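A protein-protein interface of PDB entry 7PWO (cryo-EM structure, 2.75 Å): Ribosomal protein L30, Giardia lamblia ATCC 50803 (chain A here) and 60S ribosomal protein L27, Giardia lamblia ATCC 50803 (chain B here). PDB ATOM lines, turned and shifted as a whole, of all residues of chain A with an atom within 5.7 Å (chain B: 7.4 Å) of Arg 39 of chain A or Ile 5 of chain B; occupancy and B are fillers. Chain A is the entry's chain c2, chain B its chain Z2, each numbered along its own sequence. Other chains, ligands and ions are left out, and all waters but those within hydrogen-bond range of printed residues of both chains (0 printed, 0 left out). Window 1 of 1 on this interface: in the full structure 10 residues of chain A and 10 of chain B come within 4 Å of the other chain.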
ATOM      1  N   ALA A  34      -3.796  35.267   6.073  1.00  0.00           N
ATOM      2  CA  ALA A  34      -2.979  34.228   5.457  1.00  0.00           C
ATOM      3  C   ALA A  34      -3.312  32.855   6.031  1.00  0.00           C
ATOM      4  O   ALA A  34      -3.476  31.886   5.280  1.00  0.00           O
ATOM      5  CB  ALA A  34      -1.497  34.548   5.634  1.00  0.00           C
ATOM      6  N   ILE A  35      -3.446  32.761   7.357  1.00  0.00           N
ATOM      7  CA  ILE A  35      -3.788  31.487   7.992  1.00  0.00           C
ATOM      8  C   ILE A  35      -5.167  31.009   7.562  1.00  0.00           C
ATOM      9  O   ILE A  35      -5.351  29.833   7.224  1.00  0.00           O
ATOM     10  CB  ILE A  35      -3.701  31.591   9.524  1.00  0.00           C
ATOM     11  CG1 ILE A  35      -2.269  31.883   9.968  1.00  0.00           C
ATOM     12  CG2 ILE A  35      -4.271  30.347  10.174  1.00  0.00           C
ATOM     13  CD1 ILE A  35      -2.162  32.241  11.401  1.00  0.00           C
ATOM     14  N   ARG A  36      -6.165  31.898   7.594  1.00  0.00           N
ATOM     15  CA  ARG A  36      -7.514  31.443   7.260  1.00  0.00           C
ATOM     16  C   ARG A  36      -7.573  30.923   5.825  1.00  0.00           C
ATOM     17  O   ARG A  36      -8.148  29.854   5.560  1.00  0.00           O
ATOM     18  CB  ARG A  36      -8.533  32.564   7.487  1.00  0.00           C
ATOM     19  CG  ARG A  36      -8.388  33.264   8.827  1.00  0.00           C
ATOM     20  CD  ARG A  36      -9.643  33.997   9.291  1.00  0.00           C
ATOM     21  NE  ARG A  36      -9.944  35.186   8.501  1.00  0.00           N
ATOM     22  CZ  ARG A  36      -9.823  36.440   8.929  1.00  0.00           C
ATOM     23  NH1 ARG A  36     -10.147  37.434   8.120  1.00  0.00           N
ATOM     24  NH2 ARG A  36      -9.360  36.706  10.150  1.00  0.00           N
ATOM     25  N   ASN A  37      -6.929  31.630   4.892  1.00  0.00           N
ATOM     26  CA  ASN A  37      -6.941  31.189   3.500  1.00  0.00           C
ATOM     27  C   ASN A  37      -6.142  29.903   3.291  1.00  0.00           C
ATOM     28  O   ASN A  37      -6.556  29.042   2.509  1.00  0.00           O
ATOM     29  CB  ASN A  37      -6.428  32.300   2.586  1.00  0.00           C
ATOM     30  CG  ASN A  37      -7.485  33.354   2.299  1.00  0.00           C
ATOM     31  OD1 ASN A  37      -8.679  33.056   2.215  1.00  0.00           O
ATOM     32  ND2 ASN A  37      -7.046  34.596   2.148  1.00  0.00           N
ATOM     33  N   ILE A  38      -5.000  29.743   3.965  1.00  0.00           N
ATOM     34  CA  ILE A  38      -4.264  28.488   3.821  1.00  0.00           C
ATOM     35  C   ILE A  38      -5.072  27.320   4.373  1.00  0.00           C
ATOM     36  O   ILE A  38      -5.036  26.217   3.816  1.00  0.00           O
ATOM     37  CB  ILE A  38      -2.872  28.567   4.476  1.00  0.00           C
ATOM     38  CG1 ILE A  38      -1.984  29.562   3.738  1.00  0.00           C
ATOM     39  CG2 ILE A  38      -2.183  27.213   4.448  1.00  0.00           C
ATOM     40  CD1 ILE A  38      -0.885  30.138   4.585  1.00  0.00           C
ATOM     41  N   ARG A  39      -5.822  27.530   5.467  1.00  0.00           N
ATOM     42  CA  ARG A  39      -6.669  26.438   5.938  1.00  0.00           C
ATOM     43  C   ARG A  39      -7.678  26.059   4.864  1.00  0.00           C
ATOM     44  O   ARG A  39      -7.899  24.875   4.597  1.00  0.00           O
ATOM     45  CB  ARG A  39      -7.448  26.763   7.216  1.00  0.00           C
ATOM     46  CG  ARG A  39      -6.700  26.954   8.530  1.00  0.00           C
ATOM     47  CD  ARG A  39      -7.745  27.002   9.661  1.00  0.00           C
ATOM     48  NE  ARG A  39      -8.726  28.082   9.676  1.00  0.00           N
ATOM     49  CZ  ARG A  39      -8.577  29.262  10.261  1.00  0.00           C
ATOM     50  NH1 ARG A  39      -7.484  29.545  10.954  1.00  0.00           N
ATOM     51  NH2 ARG A  39      -9.565  30.138  10.198  1.00  0.00           N
ATOM     52  N   ASP A  40      -8.307  27.058   4.242  1.00  0.00           N
ATOM     53  CA  ASP A  40      -9.316  26.750   3.236  1.00  0.00           C
ATOM     54  C   ASP A  40      -8.727  26.135   1.975  1.00  0.00           C
ATOM     55  O   ASP A  40      -9.446  25.445   1.245  1.00  0.00           O
ATOM     56  CB  ASP A  40     -10.093  28.009   2.870  1.00  0.00           C
ATOM     57  CG  ASP A  40     -10.971  28.489   3.998  1.00  0.00           C
ATOM     58  OD1 ASP A  40     -10.707  28.073   5.144  1.00  0.00           O
ATOM     59  OD2 ASP A  40     -11.905  29.285   3.737  1.00  0.00           O
ATOM     60  N   GLY A  41      -7.447  26.358   1.704  1.00  0.00           N
ATOM     61  CA  GLY A  41      -6.892  25.906   0.445  1.00  0.00           C
ATOM     62  C   GLY A  41      -7.253  26.782  -0.727  1.00  0.00           C
ATOM     63  O   GLY A  41      -7.407  26.283  -1.842  1.00  0.00           O
ATOM     64  N   LEU A  63       1.890  24.695   8.228  1.00  0.00           N
ATOM     65  CA  LEU A  63       0.562  24.711   7.634  1.00  0.00           C
ATOM     66  C   LEU A  63       0.636  24.579   6.117  1.00  0.00           C
ATOM     67  O   LEU A  63      -0.195  23.903   5.505  1.00  0.00           O
ATOM     68  CB  LEU A  63      -0.157  25.999   8.029  1.00  0.00           C
ATOM     69  CG  LEU A  63      -0.937  26.052   9.344  1.00  0.00           C
ATOM     70  CD1 LEU A  63      -1.598  27.400   9.491  1.00  0.00           C
ATOM     71  CD2 LEU A  63      -1.969  24.947   9.416  1.00  0.00           C
ATOM     72  N   LEU A  66       1.379  20.998   4.989  1.00  0.00           N
ATOM     73  CA  LEU A  66       0.155  20.196   4.971  1.00  0.00           C
ATOM     74  C   LEU A  66      -0.811  20.611   3.872  1.00  0.00           C
ATOM     75  O   LEU A  66      -1.597  19.784   3.402  1.00  0.00           O
ATOM     76  CB  LEU A  66      -0.548  20.244   6.320  1.00  0.00           C
ATOM     77  CG  LEU A  66       0.006  19.366   7.431  1.00  0.00           C
ATOM     78  CD1 LEU A  66       1.318  19.855   7.947  1.00  0.00           C
ATOM     79  CD2 LEU A  66      -1.022  19.367   8.537  1.00  0.00           C
ATOM     80  N   SER A  67      -0.797  21.874   3.465  1.00  0.00           N
ATOM     81  CA  SER A  67      -1.723  22.314   2.434  1.00  0.00           C
ATOM     82  C   SER A  67      -1.229  22.057   1.017  1.00  0.00           C
ATOM     83  O   SER A  67      -2.043  22.071   0.087  1.00  0.00           O
ATOM     84  CB  SER A  67      -2.022  23.803   2.614  1.00  0.00           C
ATOM     85  OG  SER A  67      -0.965  24.590   2.110  1.00  0.00           O
ATOM     86  N   GLN B   3      -5.097  22.286  -1.035  1.00  0.00           N
ATOM     87  CA  GLN B   3      -6.199  21.467  -0.551  1.00  0.00           C
ATOM     88  C   GLN B   3      -6.555  21.817   0.886  1.00  0.00           C
ATOM     89  O   GLN B   3      -5.681  22.169   1.680  1.00  0.00           O
ATOM     90  CB  GLN B   3      -5.841  19.979  -0.634  1.00  0.00           C
ATOM     91  CG  GLN B   3      -5.319  19.555  -1.989  1.00  0.00           C
ATOM     92  CD  GLN B   3      -5.449  18.073  -2.216  1.00  0.00           C
ATOM     93  OE1 GLN B   3      -6.462  17.601  -2.727  1.00  0.00           O
ATOM     94  NE2 GLN B   3      -4.435  17.321  -1.803  1.00  0.00           N
ATOM     95  N   PRO B   4      -7.835  21.719   1.246  1.00  0.00           N
ATOM     96  CA  PRO B   4      -8.245  22.027   2.623  1.00  0.00           C
ATOM     97  C   PRO B   4      -7.703  21.019   3.623  1.00  0.00           C
ATOM     98  O   PRO B   4      -7.469  19.852   3.303  1.00  0.00           O
ATOM     99  CB  PRO B   4      -9.775  21.969   2.561  1.00  0.00           C
ATOM    100  CG  PRO B   4     -10.107  22.112   1.103  1.00  0.00           C
ATOM    101  CD  PRO B   4      -8.987  21.491   0.359  1.00  0.00           C
ATOM    102  N   ILE B   5      -7.510  21.490   4.851  1.00  0.00           N
ATOM    103  CA  ILE B   5      -6.922  20.697   5.916  1.00  0.00           C
ATOM    104  C   ILE B   5      -7.951  20.290   6.965  1.00  0.00           C
ATOM    105  O   ILE B   5      -7.855  19.201   7.533  1.00  0.00           O
ATOM    106  CB  ILE B   5      -5.733  21.446   6.561  1.00  0.00           C
ATOM    107  CG1 ILE B   5      -4.618  21.648   5.528  1.00  0.00           C
ATOM    108  CG2 ILE B   5      -5.231  20.728   7.782  1.00  0.00           C
ATOM    109  CD1 ILE B   5      -3.506  22.589   5.966  1.00  0.00           C
ATOM    110  N   ILE B   6      -8.948  21.127   7.232  1.00  0.00           N
ATOM    111  CA  ILE B   6      -9.915  20.817   8.279  1.00  0.00           C
ATOM    112  C   ILE B   6     -10.843  19.719   7.780  1.00  0.00           C
ATOM    113  O   ILE B   6     -11.787  19.980   7.026  1.00  0.00           O
ATOM    114  CB  ILE B   6     -10.729  22.052   8.706  1.00  0.00           C
ATOM    115  CG1 ILE B   6      -9.832  23.132   9.299  1.00  0.00           C
ATOM    116  CG2 ILE B   6     -11.787  21.670   9.724  1.00  0.00           C
ATOM    117  CD1 ILE B   6      -9.293  24.084   8.274  1.00  0.00           C
ATOM    118  N   LYS B   7     -10.581  18.486   8.192  1.00  0.00           N
ATOM    119  CA  LYS B   7     -11.350  17.333   7.757  1.00  0.00           C
ATOM    120  C   LYS B   7     -11.698  16.474   8.962  1.00  0.00           C
ATOM    121  O   LYS B   7     -10.964  16.472   9.954  1.00  0.00           O
ATOM    122  CB  LYS B   7     -10.561  16.521   6.716  1.00  0.00           C
ATOM    123  CG  LYS B   7     -10.370  17.291   5.412  1.00  0.00           C
ATOM    124  CD  LYS B   7      -9.740  16.460   4.313  1.00  0.00           C
ATOM    125  CE  LYS B   7      -8.262  16.228   4.561  1.00  0.00           C
ATOM    126  NZ  LYS B   7      -7.651  15.510   3.414  1.00  0.00           N
ATOM    127  N   PRO B   8     -12.785  15.691   8.886  1.00  0.00           N
ATOM    128  CA  PRO B   8     -13.365  15.100  10.100  1.00  0.00           C
ATOM    129  C   PRO B   8     -12.599  13.934  10.709  1.00  0.00           C
ATOM    130  O   PRO B   8     -13.178  13.152  11.468  1.00  0.00           O
ATOM    131  CB  PRO B   8     -14.754  14.648   9.630  1.00  0.00           C
ATOM    132  CG  PRO B   8     -14.613  14.438   8.215  1.00  0.00           C
ATOM    133  CD  PRO B   8     -13.686  15.517   7.739  1.00  0.00           C
ATOM    134  N   GLY B   9     -11.330  13.768  10.369  1.00  0.00           N
ATOM    135  CA  GLY B   9     -10.533  12.782  11.066  1.00  0.00           C
ATOM    136  C   GLY B   9      -9.267  13.344  11.670  1.00  0.00           C
ATOM    137  O   GLY B   9      -8.417  12.595  12.154  1.00  0.00           O
ATOM    138  N   LEU B  10      -9.139  14.661  11.661  1.00  0.00           N
ATOM    139  CA  LEU B  10      -7.881  15.318  11.977  1.00  0.00           C
ATOM    140  C   LEU B  10      -7.741  15.546  13.477  1.00  0.00           C
ATOM    141  O   LEU B  10      -8.718  15.785  14.191  1.00  0.00           O
ATOM    142  CB  LEU B  10      -7.771  16.636  11.204  1.00  0.00           C
ATOM    143  CG  LEU B  10      -6.591  17.594  11.393  1.00  0.00           C
ATOM    144  CD1 LEU B  10      -5.352  17.135  10.666  1.00  0.00           C
ATOM    145  CD2 LEU B  10      -6.987  18.983  10.926  1.00  0.00           C
ATOM    146  N   CYS B  12      -6.044  17.875  16.382  1.00  0.00           N
ATOM    147  CA  CYS B  12      -5.566  19.221  16.625  1.00  0.00           C
ATOM    148  C   CYS B  12      -5.063  19.357  18.053  1.00  0.00           C
ATOM    149  O   CYS B  12      -5.386  18.552  18.932  1.00  0.00           O
ATOM    150  CB  CYS B  12      -6.666  20.251  16.369  1.00  0.00           C
ATOM    151  SG  CYS B  12      -7.030  20.579  14.637  1.00  0.00           S
ATOM    152  N   ILE B  26     -11.381  16.143  15.405  1.00  0.00           N
ATOM    153  CA  ILE B  26     -12.485  16.871  14.777  1.00  0.00           C
ATOM    154  C   ILE B  26     -13.589  15.862  14.467  1.00  0.00           C
ATOM    155  O   ILE B  26     -13.509  15.112  13.497  1.00  0.00           O
ATOM    156  CB  ILE B  26     -12.033  17.626  13.524  1.00  0.00           C
ATOM    157  CG1 ILE B  26     -11.137  18.799  13.917  1.00  0.00           C
ATOM    158  CG2 ILE B  26     -13.215  18.162  12.763  1.00  0.00           C
ATOM    159  CD1 ILE B  26      -9.992  19.028  12.957  1.00  0.00           C
ATOM    160  N   HIS B  32     -19.469  27.870   7.167  1.00  0.00           N
ATOM    161  CA  HIS B  32     -19.134  29.248   7.496  1.00  0.00           C
ATOM    162  C   HIS B  32     -20.296  30.128   7.043  1.00  0.00           C
ATOM    163  O   HIS B  32     -20.305  30.641   5.922  1.00  0.00           O
ATOM    164  CB  HIS B  32     -17.830  29.665   6.829  1.00  0.00           C
ATOM    165  CG  HIS B  32     -17.367  31.036   7.208  1.00  0.00           C
ATOM    166  ND1 HIS B  32     -18.237  32.030   7.597  1.00  0.00           N
ATOM    167  CD2 HIS B  32     -16.128  31.580   7.263  1.00  0.00           C
ATOM    168  CE1 HIS B  32     -17.554  33.125   7.874  1.00  0.00           C
ATOM    169  NE2 HIS B  32     -16.272  32.879   7.679  1.00  0.00           N
ATOM    170  N   SER B  37     -16.072  30.227  11.999  1.00  0.00           N
ATOM    171  CA  SER B  37     -15.859  28.861  11.531  1.00  0.00           C
ATOM    172  C   SER B  37     -15.621  27.963  12.731  1.00  0.00           C
ATOM    173  O   SER B  37     -14.713  28.215  13.525  1.00  0.00           O
ATOM    174  CB  SER B  37     -14.671  28.792  10.578  1.00  0.00           C
ATOM    175  OG  SER B  37     -13.473  29.094  11.254  1.00  0.00           O
ATOM    176  N   ASN B  74     -13.930  27.279  17.992  1.00  0.00           N
ATOM    177  CA  ASN B  74     -13.421  28.104  16.906  1.00  0.00           C
ATOM    178  C   ASN B  74     -12.144  27.505  16.335  1.00  0.00           C
ATOM    179  O   ASN B  74     -11.205  27.189  17.067  1.00  0.00           O
ATOM    180  CB  ASN B  74     -13.161  29.520  17.414  1.00  0.00           C
ATOM    181  CG  ASN B  74     -12.901  30.515  16.294  1.00  0.00           C
ATOM    182  OD1 ASN B  74     -12.111  31.432  16.452  1.00  0.00           O
ATOM    183  ND2 ASN B  74     -13.593  30.356  15.176  1.00  0.00           N
ATOM    184  N   VAL B  75     -12.110  27.370  15.012  1.00  0.00           N
ATOM    185  CA  VAL B  75     -10.950  26.804  14.340  1.00  0.00           C
ATOM    186  C   VAL B  75      -9.744  27.725  14.451  1.00  0.00           C
ATOM    187  O   VAL B  75      -8.600  27.262  14.386  1.00  0.00           O
ATOM    188  CB  VAL B  75     -11.304  26.493  12.875  1.00  0.00           C
ATOM    189  CG1 VAL B  75     -10.154  25.792  12.180  1.00  0.00           C
ATOM    190  CG2 VAL B  75     -12.549  25.640  12.826  1.00  0.00           C
ATOM    191  N   ASN B  76      -9.961  29.030  14.619  1.00  0.00           N
ATOM    192  CA  ASN B  76      -8.831  29.913  14.884  1.00  0.00           C
ATOM    193  C   ASN B  76      -8.135  29.576  16.195  1.00  0.00           C
ATOM    194  O   ASN B  76      -7.015  30.043  16.416  1.00  0.00           O
ATOM    195  CB  ASN B  76      -9.269  31.381  14.898  1.00  0.00           C
ATOM    196  CG  ASN B  76      -9.798  31.850  13.560  1.00  0.00           C
ATOM    197  OD1 ASN B  76     -10.975  31.703  13.252  1.00  0.00           O
ATOM    198  ND2 ASN B  76      -8.921  32.429  12.757  1.00  0.00           N
ATOM    199  N   HIS B  77      -8.770  28.786  17.065  1.00  0.00           N
ATOM    200  CA  HIS B  77      -8.157  28.301  18.294  1.00  0.00           C
ATOM    201  C   HIS B  77      -7.650  26.865  18.168  1.00  0.00           C
ATOM    202  O   HIS B  77      -7.610  26.139  19.163  1.00  0.00           O
ATOM    203  CB  HIS B  77      -9.146  28.401  19.457  1.00  0.00           C
ATOM    204  CG  HIS B  77      -9.690  29.776  19.678  1.00  0.00           C
ATOM    205  ND1 HIS B  77     -10.962  30.009  20.152  1.00  0.00           N
ATOM    206  CD2 HIS B  77      -9.132  30.994  19.489  1.00  0.00           C
ATOM    207  CE1 HIS B  77     -11.160  31.310  20.253  1.00  0.00           C
ATOM    208  NE2 HIS B  77     -10.069  31.930  19.848  1.00  0.00           N
ATOM    209  N   LEU B  78      -7.255  26.430  16.972  1.00  0.00           N
ATOM    210  CA  LEU B  78      -6.780  25.064  16.790  1.00  0.00           C
ATOM    211  C   LEU B  78      -5.491  25.053  15.980  1.00  0.00           C
ATOM    212  O   LEU B  78      -5.219  25.965  15.199  1.00  0.00           O
ATOM    213  CB  LEU B  78      -7.826  24.178  16.091  1.00  0.00           C
ATOM    214  CG  LEU B  78      -9.037  23.739  16.919  1.00  0.00           C
ATOM    215  CD1 LEU B  78     -10.270  23.661  16.044  1.00  0.00           C
ATOM    216  CD2 LEU B  78      -8.853  22.456  17.665  1.00  0.00           C
ATOM    217  N   PRO B  80      -3.706  22.153  13.556  1.00  0.00           N
ATOM    218  CA  PRO B  80      -3.750  20.798  12.987  1.00  0.00           C
ATOM    219  C   PRO B  80      -2.448  20.021  13.147  1.00  0.00           C
ATOM    220  O   PRO B  80      -1.455  20.553  13.653  1.00  0.00           O
ATOM    221  CB  PRO B  80      -4.066  21.055  11.513  1.00  0.00           C
ATOM    222  CG  PRO B  80      -3.669  22.450  11.269  1.00  0.00           C
ATOM    223  CD  PRO B  80      -3.910  23.189  12.531  1.00  0.00           C
ATOM    224  N   THR B  81      -2.449  18.755  12.725  1.00  0.00           N
ATOM    225  CA  THR B  81      -1.307  17.866  12.889  1.00  0.00           C
ATOM    226  C   THR B  81      -1.166  16.972  11.665  1.00  0.00           C
ATOM    227  O   THR B  81      -2.001  16.976  10.758  1.00  0.00           O
ATOM    228  CB  THR B  81      -1.438  16.971  14.129  1.00  0.00           C
ATOM    229  OG1 THR B  81      -2.760  16.421  14.182  1.00  0.00           O
ATOM    230  CG2 THR B  81      -1.156  17.746  15.403  1.00  0.00           C
ATOM    231  N   ARG B  84      -3.621  11.339  13.036  1.00  0.00           N
ATOM    232  CA  ARG B  84      -4.998  11.098  12.632  1.00  0.00           C
ATOM    233  C   ARG B  84      -5.581   9.944  13.435  1.00  0.00           C
ATOM    234  O   ARG B  84      -4.872   9.000  13.782  1.00  0.00           O
ATOM    235  CB  ARG B  84      -5.062  10.810  11.133  1.00  0.00           C
ATOM    236  CG  ARG B  84      -6.437  10.522  10.584  1.00  0.00           C
ATOM    237  CD  ARG B  84      -6.325  10.146   9.136  1.00  0.00           C
ATOM    238  NE  ARG B  84      -6.789  11.208   8.246  1.00  0.00           N
ATOM    239  CZ  ARG B  84      -8.056  11.582   8.110  1.00  0.00           C
ATOM    240  NH1 ARG B  84      -9.016  10.968   8.787  1.00  0.00           N
ATOM    241  NH2 ARG B  84      -8.364  12.564   7.279  1.00  0.00           N
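N of Gln 3 of chain B is in hydrogen-bond range of O of Ser 67 of chain A. The backbone NH (N) of Ile 5 of chain B is in hydrogen-bond range of the backbone carbonyl oxygen (O) of Arg 39 of chain A (3.4 Å). The side-chain amide nitrogen (ND2) of Asn 76 of chain B lies close to the guanidinium group (NH2) of Arg 39 of chain A.
O of Ser 37 of chain B lies within hydrogen-bond range of N of Val 75 of chain B (3.1 Å). The side-chain amide oxygen (OD1) of Asn 74 of chain B lies close to the side-chain amide oxygen (OD1) of Asn 76 of chain B, 3.4 Å away.
Arg 36 of chain A touches Asn 76 of chain B (CD to ND2, 3.9 Å). Pro 4 of chain B touches Arg 39 of chain A (CA to O, 3.5 Å). CB of Arg 39 of chain A touches CD1 of Ile 6 of chain B, 3.4 Å away. Val 75 of chain B touches Arg 39 of chain A. O of Asp 40 of chain A touches CG of Pro 4 of chain B (3.4 Å). Ile 5 of chain B touches Leu 63 of chain A (CD1 to O, 3.6 Å). Pro 80 of chain B touches Leu 63 of chain A (CG to CD2, 3.5 Å). Ile 5 of chain B touches Leu 66 of chain A (CD1 to CB, 3.8 Å). Leu 66 of chain A touches Thr 81 of chain B (CD2 to O, 3.4 Å). Ser 67 of chain A touches Ile 5 of chain B.
Ala 34 of chain A touches none of the printed residues of chain B. Of the printed residues of chain B, Arg 39 of chain A touches Pro 4, Ile 5, Ile 6, Val 75 and Asn 76. Printed residues of chain B within 4 Å of Leu 63 of chain A: Ile 5 and Pro 80. Of chain A, only Arg 39 (3.4 Å), Leu 63 (3.6 Å), Leu 66 (3.8 Å) and Ser 67 (3.8 Å) come within 4 Å of Ile 5 of chain B. Printed residues of chain A within 4 Å of Ile 6 of chain B: Arg 39. Leu 10 of chain B touches none of the printed residues of chain A. Of the printed residues of chain A, Asn 76 of chain B touches Arg 36 (3.9 Å) and Arg 39 (3.5 Å). The nearest residue of chain B that does not touch Arg 39 of chain A is Ser 37 of chain B (4.2 Å). The nearest residue of chain A that does not touch Ile 5 of chain B is Ile 38 of chain A (4.5 Å). The nearest printed residue of chain A that does not touch Pro 4 of chain B is Gly 41 of chain A (4.4 Å).
Of the 20 printed residues of chain B, 8 touch a printed residue of chain A. Hydrophobic or aromatic side chains of chain B that line the printed part of chain A: Pro 4, Ile 5, Ile 6, Val 75 and Pro 80. Along chain B the printed residues that touch a printed residue of chain A span positions 3 to 81. Among the printed residues, 13 pairs touch across the chains. Among the printed residues, no Asp or Glu carboxylate lies within 4 Å of a Lys or Arg side-chain nitrogen of the other chain.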
